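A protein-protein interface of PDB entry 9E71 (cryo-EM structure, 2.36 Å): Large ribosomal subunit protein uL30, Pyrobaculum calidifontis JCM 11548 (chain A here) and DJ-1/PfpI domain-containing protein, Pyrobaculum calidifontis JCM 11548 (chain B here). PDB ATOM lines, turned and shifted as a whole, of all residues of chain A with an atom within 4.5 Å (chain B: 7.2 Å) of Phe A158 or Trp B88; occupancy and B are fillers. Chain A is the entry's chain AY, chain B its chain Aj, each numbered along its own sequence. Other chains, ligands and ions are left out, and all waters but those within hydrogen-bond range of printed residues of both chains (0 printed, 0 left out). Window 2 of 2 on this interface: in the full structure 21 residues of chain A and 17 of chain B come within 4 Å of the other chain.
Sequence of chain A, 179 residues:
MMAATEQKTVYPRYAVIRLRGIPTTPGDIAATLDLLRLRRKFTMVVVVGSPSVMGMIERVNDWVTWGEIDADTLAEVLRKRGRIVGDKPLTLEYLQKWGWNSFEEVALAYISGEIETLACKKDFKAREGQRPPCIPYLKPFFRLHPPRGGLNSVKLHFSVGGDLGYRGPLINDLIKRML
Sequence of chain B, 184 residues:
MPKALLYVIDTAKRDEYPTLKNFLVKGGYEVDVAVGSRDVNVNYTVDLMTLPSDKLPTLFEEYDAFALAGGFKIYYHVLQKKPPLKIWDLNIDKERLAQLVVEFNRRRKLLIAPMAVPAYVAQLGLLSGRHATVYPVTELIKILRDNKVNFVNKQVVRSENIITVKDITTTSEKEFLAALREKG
Of chain B, only Leu B85 (3.7 Å) and Trp B88 (3.8 Å) come within 4 Å of Phe A158. Of the printed residues of chain B, Tyr A166 touches Tyr B76 (2.7 Å), Lys B81 (3.8 Å) and Pro B84 (3.5 Å). Of the printed residues of chain B, Arg A167 touches Trp B88. Of the printed residues of chain A, Tyr B75 touches Pro A169. Printed residues of chain A within 4 Å of Leu B85: Phe A158 (3.7 Å) and Ser A159 (3.5 Å). Of chain A, only Phe A158 (3.8 Å), Arg A167 (3.7 Å) and Leu A170 (3.5 Å) come within 4 Å of Trp B88. The nearest residue of chain B that does not touch Phe A158 is Pro B84 (4.5 Å). The nearest residue of chain A that does not touch Trp B88 is Pro A169 (4.3 Å).
Of the 13 printed residues of chain A, 6 touch a printed residue of chain B. Along chain A the printed residues that touch a printed residue of chain B span positions 158 to 170. Printed residues of chain B that touch a printed residue of chain A: Phe B72, Tyr B75, Tyr B76, Lys B81, Pro B84, Leu B85 and Trp B88. Hydrophobic or aromatic side chains of chain B that line the printed part of chain A: Phe B72, Tyr B75, Tyr B76, Pro B84, Leu B85 and Trp B88. Among the printed residues, 13 pairs touch across the chains.
The backbone NH of Phe A158 lies within hydrogen-bond range of the backbone carbonyl oxygen of Leu A164, at 2.6 Å. OD2 of Asp A163 lies within salt-bridge range of NH2 of Arg A167 (3.0 Å). The backbone NH (N) of Lys B81 lies within hydrogen-bond range of the backbone carbonyl oxygen (O) of Tyr B76, at 3.2 Å.
Among the printed residues, pairs that only touch across the chains: Phe A158 with Leu B85 (3.7 Å), Phe A158 with Trp B88 (3.8 Å), Ser A159 with Pro B84 (3.5 Å), Ser A159 with Leu B85 (3.5 Å), Tyr A166 with Lys B81 (3.8 Å), Tyr A166 with Pro B84 (3.5 Å), Arg A167 with Trp B88 (3.7 Å), Pro A169 with Phe B72 (3.8 Å), Pro A169 with Tyr B75 (3.6 Å), Pro A169 with Tyr B76 (3.7 Å), Leu A170 with Phe B72 (3.4 Å) and Leu A170 with Trp B88 (3.5 Å).
OH of Tyr B76 sits at hydrogen-bond distance from OH of Tyr A166, at 2.7 Å.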
ATOM      1  N   LEU A 156     -10.484   3.759 -10.908  1.00  0.00           N
ATOM      2  CA  LEU A 156     -10.203   3.811 -12.332  1.00  0.00           C
ATOM      3  C   LEU A 156      -9.996   5.248 -12.780  1.00  0.00           C
ATOM      4  O   LEU A 156     -10.517   6.187 -12.177  1.00  0.00           O
ATOM      5  CB  LEU A 156     -11.325   3.180 -13.151  1.00  0.00           C
ATOM      6  CG  LEU A 156     -11.685   1.739 -12.814  1.00  0.00           C
ATOM      7  CD1 LEU A 156     -12.944   1.329 -13.552  1.00  0.00           C
ATOM      8  CD2 LEU A 156     -10.535   0.818 -13.152  1.00  0.00           C
ATOM      9  N   HIS A 157      -9.224   5.409 -13.846  1.00  0.00           N
ATOM     10  CA  HIS A 157      -8.961   6.729 -14.390  1.00  0.00           C
ATOM     11  C   HIS A 157     -10.201   7.274 -15.082  1.00  0.00           C
ATOM     12  O   HIS A 157     -11.042   6.524 -15.578  1.00  0.00           O
ATOM     13  CB  HIS A 157      -7.798   6.671 -15.375  1.00  0.00           C
ATOM     14  CG  HIS A 157      -6.455   6.654 -14.719  1.00  0.00           C
ATOM     15  ND1 HIS A 157      -5.293   6.954 -15.393  1.00  0.00           N
ATOM     16  CD2 HIS A 157      -6.090   6.382 -13.444  1.00  0.00           C
ATOM     17  CE1 HIS A 157      -4.269   6.861 -14.565  1.00  0.00           C
ATOM     18  NE2 HIS A 157      -4.726   6.516 -13.375  1.00  0.00           N
ATOM     19  N   PHE A 158     -10.304   8.604 -15.119  1.00  0.00           N
ATOM     20  CA  PHE A 158     -11.398   9.243 -15.841  1.00  0.00           C
ATOM     21  C   PHE A 158     -11.341   8.934 -17.328  1.00  0.00           C
ATOM     22  O   PHE A 158     -12.383   8.846 -17.985  1.00  0.00           O
ATOM     23  CB  PHE A 158     -11.361  10.752 -15.613  1.00  0.00           C
ATOM     24  CG  PHE A 158     -12.392  11.510 -16.392  1.00  0.00           C
ATOM     25  CD1 PHE A 158     -13.711  11.528 -15.983  1.00  0.00           C
ATOM     26  CD2 PHE A 158     -12.041  12.215 -17.525  1.00  0.00           C
ATOM     27  CE1 PHE A 158     -14.656  12.227 -16.693  1.00  0.00           C
ATOM     28  CE2 PHE A 158     -12.984  12.915 -18.237  1.00  0.00           C
ATOM     29  CZ  PHE A 158     -14.292  12.921 -17.821  1.00  0.00           C
ATOM     30  N   SER A 159     -10.141   8.748 -17.873  1.00  0.00           N
ATOM     31  CA  SER A 159      -9.974   8.453 -19.287  1.00  0.00           C
ATOM     32  C   SER A 159     -10.435   7.054 -19.669  1.00  0.00           C
ATOM     33  O   SER A 159     -10.527   6.762 -20.865  1.00  0.00           O
ATOM     34  CB  SER A 159      -8.511   8.635 -19.677  1.00  0.00           C
ATOM     35  OG  SER A 159      -7.658   8.015 -18.734  1.00  0.00           O
ATOM     36  N   VAL A 160     -10.709   6.184 -18.701  1.00  0.00           N
ATOM     37  CA  VAL A 160     -11.228   4.852 -18.971  1.00  0.00           C
ATOM     38  C   VAL A 160     -12.637   4.669 -18.428  1.00  0.00           C
ATOM     39  O   VAL A 160     -13.122   3.544 -18.342  1.00  0.00           O
ATOM     40  CB  VAL A 160     -10.287   3.765 -18.419  1.00  0.00           C
ATOM     41  CG1 VAL A 160      -9.034   3.684 -19.259  1.00  0.00           C
ATOM     42  CG2 VAL A 160      -9.941   4.056 -16.976  1.00  0.00           C
ATOM     43  N   GLY A 161     -13.308   5.757 -18.069  1.00  0.00           N
ATOM     44  CA  GLY A 161     -14.632   5.685 -17.497  1.00  0.00           C
ATOM     45  C   GLY A 161     -14.685   5.783 -15.991  1.00  0.00           C
ATOM     46  O   GLY A 161     -15.783   5.747 -15.425  1.00  0.00           O
ATOM     47  N   GLY A 162     -13.550   5.905 -15.326  1.00  0.00           N
ATOM     48  CA  GLY A 162     -13.501   6.054 -13.889  1.00  0.00           C
ATOM     49  C   GLY A 162     -13.590   7.501 -13.471  1.00  0.00           C
ATOM     50  O   GLY A 162     -14.196   8.335 -14.150  1.00  0.00           O
ATOM     51  N   ASP A 163     -12.968   7.811 -12.338  1.00  0.00           N
ATOM     52  CA  ASP A 163     -13.030   9.144 -11.769  1.00  0.00           C
ATOM     53  C   ASP A 163     -11.677   9.797 -11.547  1.00  0.00           C
ATOM     54  O   ASP A 163     -11.629  11.019 -11.387  1.00  0.00           O
ATOM     55  CB  ASP A 163     -13.778   9.107 -10.433  1.00  0.00           C
ATOM     56  CG  ASP A 163     -15.255   8.864 -10.609  1.00  0.00           C
ATOM     57  OD1 ASP A 163     -15.739   7.820 -10.130  1.00  0.00           O
ATOM     58  OD2 ASP A 163     -15.934   9.718 -11.218  1.00  0.00           O
ATOM     59  N   LEU A 164     -10.590   9.037 -11.542  1.00  0.00           N
ATOM     60  CA  LEU A 164      -9.299   9.580 -11.159  1.00  0.00           C
ATOM     61  C   LEU A 164      -8.628  10.289 -12.328  1.00  0.00           C
ATOM     62  O   LEU A 164      -8.896  10.013 -13.498  1.00  0.00           O
ATOM     63  CB  LEU A 164      -8.386   8.474 -10.645  1.00  0.00           C
ATOM     64  CG  LEU A 164      -8.844   7.727  -9.398  1.00  0.00           C
ATOM     65  CD1 LEU A 164      -8.035   6.463  -9.231  1.00  0.00           C
ATOM     66  CD2 LEU A 164      -8.717   8.617  -8.184  1.00  0.00           C
ATOM     67  N   TYR A 166      -6.873  13.572 -14.625  1.00  0.00           N
ATOM     68  CA  TYR A 166      -7.267  14.830 -15.239  1.00  0.00           C
ATOM     69  C   TYR A 166      -8.689  14.733 -15.768  1.00  0.00           C
ATOM     70  O   TYR A 166      -9.026  13.813 -16.517  1.00  0.00           O
ATOM     71  CB  TYR A 166      -6.304  15.187 -16.366  1.00  0.00           C
ATOM     72  CG  TYR A 166      -6.635  16.469 -17.080  1.00  0.00           C
ATOM     73  CD1 TYR A 166      -6.794  17.652 -16.383  1.00  0.00           C
ATOM     74  CD2 TYR A 166      -6.776  16.499 -18.455  1.00  0.00           C
ATOM     75  CE1 TYR A 166      -7.088  18.823 -17.033  1.00  0.00           C
ATOM     76  CE2 TYR A 166      -7.070  17.662 -19.114  1.00  0.00           C
ATOM     77  CZ  TYR A 166      -7.225  18.822 -18.401  1.00  0.00           C
ATOM     78  OH  TYR A 166      -7.522  19.986 -19.066  1.00  0.00           O
ATOM     79  N   ARG A 167      -9.517  15.696 -15.388  1.00  0.00           N
ATOM     80  CA  ARG A 167     -10.938  15.681 -15.690  1.00  0.00           C
ATOM     81  C   ARG A 167     -11.338  16.779 -16.661  1.00  0.00           C
ATOM     82  O   ARG A 167     -12.471  16.779 -17.145  1.00  0.00           O
ATOM     83  CB  ARG A 167     -11.732  15.815 -14.384  1.00  0.00           C
ATOM     84  CG  ARG A 167     -13.211  15.570 -14.496  1.00  0.00           C
ATOM     85  CD  ARG A 167     -13.845  15.474 -13.126  1.00  0.00           C
ATOM     86  NE  ARG A 167     -13.626  14.166 -12.526  1.00  0.00           N
ATOM     87  CZ  ARG A 167     -14.573  13.258 -12.357  1.00  0.00           C
ATOM     88  NH1 ARG A 167     -15.821  13.486 -12.725  1.00  0.00           N
ATOM     89  NH2 ARG A 167     -14.260  12.092 -11.805  1.00  0.00           N
ATOM     90  N   PRO A 169     -12.604  20.409 -17.844  1.00  0.00           N
ATOM     91  CA  PRO A 169     -13.559  21.343 -17.239  1.00  0.00           C
ATOM     92  C   PRO A 169     -14.737  20.671 -16.554  1.00  0.00           C
ATOM     93  O   PRO A 169     -15.598  21.374 -16.017  1.00  0.00           O
ATOM     94  CB  PRO A 169     -14.027  22.185 -18.438  1.00  0.00           C
ATOM     95  CG  PRO A 169     -13.321  21.640 -19.645  1.00  0.00           C
ATOM     96  CD  PRO A 169     -12.783  20.305 -19.296  1.00  0.00           C
ATOM     97  N   LEU A 170     -14.798  19.337 -16.544  1.00  0.00           N
ATOM     98  CA  LEU A 170     -15.836  18.613 -15.819  1.00  0.00           C
ATOM     99  C   LEU A 170     -15.630  18.639 -14.312  1.00  0.00           C
ATOM    100  O   LEU A 170     -16.524  18.212 -13.566  1.00  0.00           O
ATOM    101  CB  LEU A 170     -15.897  17.169 -16.308  1.00  0.00           C
ATOM    102  CG  LEU A 170     -16.565  16.962 -17.666  1.00  0.00           C
ATOM    103  CD1 LEU A 170     -16.479  15.513 -18.089  1.00  0.00           C
ATOM    104  CD2 LEU A 170     -18.004  17.413 -17.611  1.00  0.00           C
ATOM    105  N   ASP B  10     -20.916  18.616 -30.346  1.00  0.00           N
ATOM    106  CA  ASP B  10     -20.599  17.612 -29.344  1.00  0.00           C
ATOM    107  C   ASP B  10     -21.758  17.463 -28.374  1.00  0.00           C
ATOM    108  O   ASP B  10     -22.428  18.438 -28.026  1.00  0.00           O
ATOM    109  CB  ASP B  10     -19.325  17.972 -28.576  1.00  0.00           C
ATOM    110  CG  ASP B  10     -18.632  16.758 -28.001  1.00  0.00           C
ATOM    111  OD1 ASP B  10     -19.330  15.797 -27.621  1.00  0.00           O
ATOM    112  OD2 ASP B  10     -17.389  16.761 -27.923  1.00  0.00           O
ATOM    113  N   ALA B  12     -20.962  15.902 -25.428  1.00  0.00           N
ATOM    114  CA  ALA B  12     -20.243  15.604 -24.195  1.00  0.00           C
ATOM    115  C   ALA B  12     -20.811  16.392 -23.022  1.00  0.00           C
ATOM    116  O   ALA B  12     -20.947  15.860 -21.914  1.00  0.00           O
ATOM    117  CB  ALA B  12     -18.755  15.897 -24.376  1.00  0.00           C
ATOM    118  N   LYS B  13     -21.142  17.658 -23.242  1.00  0.00           N
ATOM    119  CA  LYS B  13     -21.906  18.432 -22.269  1.00  0.00           C
ATOM    120  C   LYS B  13     -23.352  17.971 -22.386  1.00  0.00           C
ATOM    121  O   LYS B  13     -24.025  18.253 -23.379  1.00  0.00           O
ATOM    122  CB  LYS B  13     -21.752  19.924 -22.531  1.00  0.00           C
ATOM    123  CG  LYS B  13     -22.165  20.800 -21.370  1.00  0.00           C
ATOM    124  CD  LYS B  13     -21.066  20.890 -20.332  1.00  0.00           C
ATOM    125  CE  LYS B  13     -21.087  22.232 -19.622  1.00  0.00           C
ATOM    126  NZ  LYS B  13     -21.262  22.073 -18.155  1.00  0.00           N
ATOM    127  N   ASP B  39     -20.392  10.759 -34.235  1.00  0.00           N
ATOM    128  CA  ASP B  39     -20.429  10.416 -32.822  1.00  0.00           C
ATOM    129  C   ASP B  39     -21.543  11.119 -32.059  1.00  0.00           C
ATOM    130  O   ASP B  39     -21.620  10.972 -30.836  1.00  0.00           O
ATOM    131  CB  ASP B  39     -19.084  10.739 -32.170  1.00  0.00           C
ATOM    132  CG  ASP B  39     -18.961  12.194 -31.788  1.00  0.00           C
ATOM    133  OD1 ASP B  39     -19.072  13.053 -32.684  1.00  0.00           O
ATOM    134  OD2 ASP B  39     -18.757  12.480 -30.591  1.00  0.00           O
ATOM    135  N   GLY B  71     -19.230  21.481 -27.074  1.00  0.00           N
ATOM    136  CA  GLY B  71     -18.876  21.117 -25.718  1.00  0.00           C
ATOM    137  C   GLY B  71     -17.393  21.258 -25.473  1.00  0.00           C
ATOM    138  O   GLY B  71     -16.854  22.365 -25.529  1.00  0.00           O
ATOM    139  N   PHE B  72     -16.720  20.144 -25.193  1.00  0.00           N
ATOM    140  CA  PHE B  72     -15.288  20.184 -24.939  1.00  0.00           C
ATOM    141  C   PHE B  72     -14.450  20.046 -26.200  1.00  0.00           C
ATOM    142  O   PHE B  72     -13.243  20.302 -26.146  1.00  0.00           O
ATOM    143  CB  PHE B  72     -14.913  19.094 -23.939  1.00  0.00           C
ATOM    144  CG  PHE B  72     -15.858  18.999 -22.784  1.00  0.00           C
ATOM    145  CD1 PHE B  72     -15.994  20.055 -21.903  1.00  0.00           C
ATOM    146  CD2 PHE B  72     -16.621  17.865 -22.586  1.00  0.00           C
ATOM    147  CE1 PHE B  72     -16.863  19.978 -20.840  1.00  0.00           C
ATOM    148  CE2 PHE B  72     -17.493  17.783 -21.523  1.00  0.00           C
ATOM    149  CZ  PHE B  72     -17.615  18.843 -20.650  1.00  0.00           C
ATOM    150  N   LYS B  73     -15.057  19.659 -27.325  1.00  0.00           N
ATOM    151  CA  LYS B  73     -14.330  19.617 -28.591  1.00  0.00           C
ATOM    152  C   LYS B  73     -13.816  20.999 -28.965  1.00  0.00           C
ATOM    153  O   LYS B  73     -12.623  21.182 -29.247  1.00  0.00           O
ATOM    154  CB  LYS B  73     -15.234  19.076 -29.695  1.00  0.00           C
ATOM    155  CG  LYS B  73     -15.231  17.577 -29.827  1.00  0.00           C
ATOM    156  CD  LYS B  73     -16.214  17.139 -30.893  1.00  0.00           C
ATOM    157  CE  LYS B  73     -16.618  15.691 -30.729  1.00  0.00           C
ATOM    158  NZ  LYS B  73     -18.051  15.496 -31.061  1.00  0.00           N
ATOM    159  N   ILE B  74     -14.703  21.991 -28.928  1.00  0.00           N
ATOM    160  CA  ILE B  74     -14.315  23.361 -29.232  1.00  0.00           C
ATOM    161  C   ILE B  74     -13.348  23.887 -28.186  1.00  0.00           C
ATOM    162  O   ILE B  74     -12.429  24.647 -28.506  1.00  0.00           O
ATOM    163  CB  ILE B  74     -15.563  24.250 -29.356  1.00  0.00           C
ATOM    164  CG1 ILE B  74     -16.266  23.964 -30.682  1.00  0.00           C
ATOM    165  CG2 ILE B  74     -15.188  25.715 -29.247  1.00  0.00           C
ATOM    166  CD1 ILE B  74     -15.337  23.993 -31.869  1.00  0.00           C
ATOM    167  N   TYR B  75     -13.528  23.479 -26.927  1.00  0.00           N
ATOM    168  CA  TYR B  75     -12.672  23.969 -25.851  1.00  0.00           C
ATOM    169  C   TYR B  75     -11.234  23.512 -26.056  1.00  0.00           C
ATOM    170  O   TYR B  75     -10.299  24.319 -26.014  1.00  0.00           O
ATOM    171  CB  TYR B  75     -13.257  23.523 -24.494  1.00  0.00           C
ATOM    172  CG  TYR B  75     -12.384  23.625 -23.240  1.00  0.00           C
ATOM    173  CD1 TYR B  75     -11.408  22.676 -22.929  1.00  0.00           C
ATOM    174  CD2 TYR B  75     -12.534  24.698 -22.375  1.00  0.00           C
ATOM    175  CE1 TYR B  75     -10.631  22.798 -21.817  1.00  0.00           C
ATOM    176  CE2 TYR B  75     -11.758  24.819 -21.253  1.00  0.00           C
ATOM    177  CZ  TYR B  75     -10.808  23.864 -20.982  1.00  0.00           C
ATOM    178  OH  TYR B  75     -10.022  23.972 -19.866  1.00  0.00           O
ATOM    179  N   TYR B  76     -11.035  22.217 -26.273  1.00  0.00           N
ATOM    180  CA  TYR B  76      -9.675  21.737 -26.431  1.00  0.00           C
ATOM    181  C   TYR B  76      -9.087  22.105 -27.781  1.00  0.00           C
ATOM    182  O   TYR B  76      -7.864  22.235 -27.886  1.00  0.00           O
ATOM    183  CB  TYR B  76      -9.616  20.231 -26.184  1.00  0.00           C
ATOM    184  CG  TYR B  76      -9.602  19.920 -24.705  1.00  0.00           C
ATOM    185  CD1 TYR B  76      -8.470  20.157 -23.940  1.00  0.00           C
ATOM    186  CD2 TYR B  76     -10.728  19.424 -24.066  1.00  0.00           C
ATOM    187  CE1 TYR B  76      -8.454  19.891 -22.587  1.00  0.00           C
ATOM    188  CE2 TYR B  76     -10.720  19.155 -22.716  1.00  0.00           C
ATOM    189  CZ  TYR B  76      -9.581  19.391 -21.980  1.00  0.00           C
ATOM    190  OH  TYR B  76      -9.572  19.123 -20.635  1.00  0.00           O
ATOM    191  N   HIS B  77      -9.914  22.321 -28.807  1.00  0.00           N
ATOM    192  CA  HIS B  77      -9.372  22.857 -30.049  1.00  0.00           C
ATOM    193  C   HIS B  77      -8.875  24.286 -29.862  1.00  0.00           C
ATOM    194  O   HIS B  77      -7.801  24.648 -30.350  1.00  0.00           O
ATOM    195  CB  HIS B  77     -10.415  22.805 -31.155  1.00  0.00           C
ATOM    196  CG  HIS B  77     -10.016  23.571 -32.374  1.00  0.00           C
ATOM    197  ND1 HIS B  77     -10.596  24.770 -32.722  1.00  0.00           N
ATOM    198  CD2 HIS B  77      -9.078  23.319 -33.314  1.00  0.00           C
ATOM    199  CE1 HIS B  77     -10.038  25.219 -33.831  1.00  0.00           C
ATOM    200  NE2 HIS B  77      -9.114  24.357 -34.211  1.00  0.00           N
ATOM    201  N   LYS B  81      -4.830  21.789 -26.989  1.00  0.00           N
ATOM    202  CA  LYS B  81      -4.342  20.843 -26.002  1.00  0.00           C
ATOM    203  C   LYS B  81      -4.986  19.484 -26.224  1.00  0.00           C
ATOM    204  O   LYS B  81      -6.130  19.385 -26.671  1.00  0.00           O
ATOM    205  CB  LYS B  81      -4.635  21.329 -24.579  1.00  0.00           C
ATOM    206  CG  LYS B  81      -3.446  21.962 -23.892  1.00  0.00           C
ATOM    207  CD  LYS B  81      -3.863  22.757 -22.670  1.00  0.00           C
ATOM    208  CE  LYS B  81      -5.036  22.107 -21.953  1.00  0.00           C
ATOM    209  NZ  LYS B  81      -4.711  20.752 -21.433  1.00  0.00           N
ATOM    210  N   LYS B  82      -4.244  18.444 -25.899  1.00  0.00           N
ATOM    211  CA  LYS B  82      -4.767  17.093 -26.023  1.00  0.00           C
ATOM    212  C   LYS B  82      -5.822  16.863 -24.942  1.00  0.00           C
ATOM    213  O   LYS B  82      -5.525  17.025 -23.754  1.00  0.00           O
ATOM    214  CB  LYS B  82      -3.618  16.092 -25.889  1.00  0.00           C
ATOM    215  CG  LYS B  82      -3.905  14.695 -26.398  1.00  0.00           C
ATOM    216  CD  LYS B  82      -4.737  14.734 -27.670  1.00  0.00           C
ATOM    217  CE  LYS B  82      -5.594  13.482 -27.815  1.00  0.00           C
ATOM    218  NZ  LYS B  82      -6.840  13.711 -28.613  1.00  0.00           N
ATOM    219  N   PRO B  83      -7.049  16.498 -25.299  1.00  0.00           N
ATOM    220  CA  PRO B  83      -8.080  16.279 -24.288  1.00  0.00           C
ATOM    221  C   PRO B  83      -7.876  14.952 -23.583  1.00  0.00           C
ATOM    222  O   PRO B  83      -7.254  14.040 -24.142  1.00  0.00           O
ATOM    223  CB  PRO B  83      -9.382  16.287 -25.101  1.00  0.00           C
ATOM    224  CG  PRO B  83      -8.985  16.103 -26.523  1.00  0.00           C
ATOM    225  CD  PRO B  83      -7.505  16.104 -26.639  1.00  0.00           C
ATOM    226  N   PRO B  84      -8.389  14.798 -22.357  1.00  0.00           N
ATOM    227  CA  PRO B  84      -8.229  13.515 -21.647  1.00  0.00           C
ATOM    228  C   PRO B  84      -8.914  12.336 -22.322  1.00  0.00           C
ATOM    229  O   PRO B  84      -8.525  11.191 -22.063  1.00  0.00           O
ATOM    230  CB  PRO B  84      -8.833  13.782 -20.263  1.00  0.00           C
ATOM    231  CG  PRO B  84      -9.443  15.125 -20.307  1.00  0.00           C
ATOM    232  CD  PRO B  84      -9.273  15.736 -21.650  1.00  0.00           C
ATOM    233  N   LEU B  85      -9.900  12.569 -23.181  1.00  0.00           N
ATOM    234  CA  LEU B  85     -10.627  11.505 -23.856  1.00  0.00           C
ATOM    235  C   LEU B  85     -10.448  11.656 -25.355  1.00  0.00           C
ATOM    236  O   LEU B  85     -10.432  12.778 -25.866  1.00  0.00           O
ATOM    237  CB  LEU B  85     -12.110  11.541 -23.488  1.00  0.00           C
ATOM    238  CG  LEU B  85     -12.392  11.261 -22.014  1.00  0.00           C
ATOM    239  CD1 LEU B  85     -13.801  11.664 -21.637  1.00  0.00           C
ATOM    240  CD2 LEU B  85     -12.171   9.787 -21.725  1.00  0.00           C
ATOM    241  N   LYS B  86     -10.313  10.528 -26.056  1.00  0.00           N
ATOM    242  CA  LYS B  86     -10.182  10.579 -27.510  1.00  0.00           C
ATOM    243  C   LYS B  86     -11.451  11.111 -28.158  1.00  0.00           C
ATOM    244  O   LYS B  86     -11.394  11.675 -29.255  1.00  0.00           O
ATOM    245  CB  LYS B  86      -9.796   9.181 -28.035  1.00  0.00           C
ATOM    246  CG  LYS B  86      -9.661   8.875 -29.578  1.00  0.00           C
ATOM    247  CD  LYS B  86     -10.937   8.938 -30.442  1.00  0.00           C
ATOM    248  CE  LYS B  86     -11.766   7.681 -30.304  1.00  0.00           C
ATOM    249  NZ  LYS B  86     -13.073   7.829 -31.001  1.00  0.00           N
ATOM    250  N   ILE B  87     -12.605  10.912 -27.520  1.00  0.00           N
ATOM    251  CA  ILE B  87     -13.868  11.347 -28.094  1.00  0.00           C
ATOM    252  C   ILE B  87     -14.136  12.826 -27.877  1.00  0.00           C
ATOM    253  O   ILE B  87     -15.202  13.314 -28.263  1.00  0.00           O
ATOM    254  CB  ILE B  87     -15.005  10.492 -27.509  1.00  0.00           C
ATOM    255  CG1 ILE B  87     -15.088  10.686 -25.997  1.00  0.00           C
ATOM    256  CG2 ILE B  87     -14.772   9.034 -27.828  1.00  0.00           C
ATOM    257  CD1 ILE B  87     -16.294  11.453 -25.558  1.00  0.00           C
ATOM    258  N   TRP B  88     -13.206  13.549 -27.267  1.00  0.00           N
ATOM    259  CA  TRP B  88     -13.346  14.981 -27.068  1.00  0.00           C
ATOM    260  C   TRP B  88     -12.662  15.806 -28.146  1.00  0.00           C
ATOM    261  O   TRP B  88     -12.713  17.036 -28.081  1.00  0.00           O
ATOM    262  CB  TRP B  88     -12.788  15.385 -25.703  1.00  0.00           C
ATOM    263  CG  TRP B  88     -13.691  15.077 -24.562  1.00  0.00           C
ATOM    264  CD1 TRP B  88     -14.839  14.352 -24.601  1.00  0.00           C
ATOM    265  CD2 TRP B  88     -13.522  15.491 -23.204  1.00  0.00           C
ATOM    266  NE1 TRP B  88     -15.397  14.283 -23.352  1.00  0.00           N
ATOM    267  CE2 TRP B  88     -14.606  14.976 -22.475  1.00  0.00           C
ATOM    268  CE3 TRP B  88     -12.556  16.246 -22.535  1.00  0.00           C
ATOM    269  CZ2 TRP B  88     -14.754  15.190 -21.110  1.00  0.00           C
ATOM    270  CZ3 TRP B  88     -12.704  16.461 -21.179  1.00  0.00           C
ATOM    271  CH2 TRP B  88     -13.796  15.935 -20.481  1.00  0.00           C
ATOM    272  N   ASP B  89     -12.017  15.176 -29.124  1.00  0.00           N
ATOM    273  CA  ASP B  89     -11.332  15.943 -30.152  1.00  0.00           C
ATOM    274  C   ASP B  89     -12.309  16.450 -31.206  1.00  0.00           C
ATOM    275  O   ASP B  89     -13.350  15.843 -31.469  1.00  0.00           O
ATOM    276  CB  ASP B  89     -10.234  15.112 -30.815  1.00  0.00           C
ATOM    277  CG  ASP B  89     -10.730  13.777 -31.332  1.00  0.00           C
ATOM    278  OD1 ASP B  89     -11.942  13.500 -31.244  1.00  0.00           O
ATOM    279  OD2 ASP B  89      -9.903  13.000 -31.853  1.00  0.00           O
ATOM    280  N   LEU B  90     -11.954  17.569 -31.824  1.00  0.00           N
ATOM    281  CA  LEU B  90     -12.762  18.153 -32.888  1.00  0.00           C
ATOM    282  C   LEU B  90     -12.671  17.259 -34.116  1.00  0.00           C
ATOM    283  O   LEU B  90     -11.684  17.291 -34.853  1.00  0.00           O
ATOM    284  CB  LEU B  90     -12.286  19.566 -33.197  1.00  0.00           C
ATOM    285  CG  LEU B  90     -13.203  20.369 -34.113  1.00  0.00           C
ATOM    286  CD1 LEU B  90     -14.586  20.448 -33.509  1.00  0.00           C
ATOM    287  CD2 LEU B  90     -12.640  21.753 -34.352  1.00  0.00           C
ATOM    288  N   ASN B  91     -13.706  16.450 -34.344  1.00  0.00           N
ATOM    289  CA  ASN B  91     -13.745  15.518 -35.465  1.00  0.00           C
ATOM    290  C   ASN B  91     -14.672  15.989 -36.580  1.00  0.00           C
ATOM    291  O   ASN B  91     -15.188  15.168 -37.346  1.00  0.00           O
ATOM    292  CB  ASN B  91     -14.163  14.129 -34.987  1.00  0.00           C
ATOM    293  CG  ASN B  91     -15.396  14.163 -34.113  1.00  0.00           C
ATOM    294  OD1 ASN B  91     -16.037  15.201 -33.967  1.00  0.00           O
ATOM    295  ND2 ASN B  91     -15.739  13.022 -33.529  1.00  0.00           N
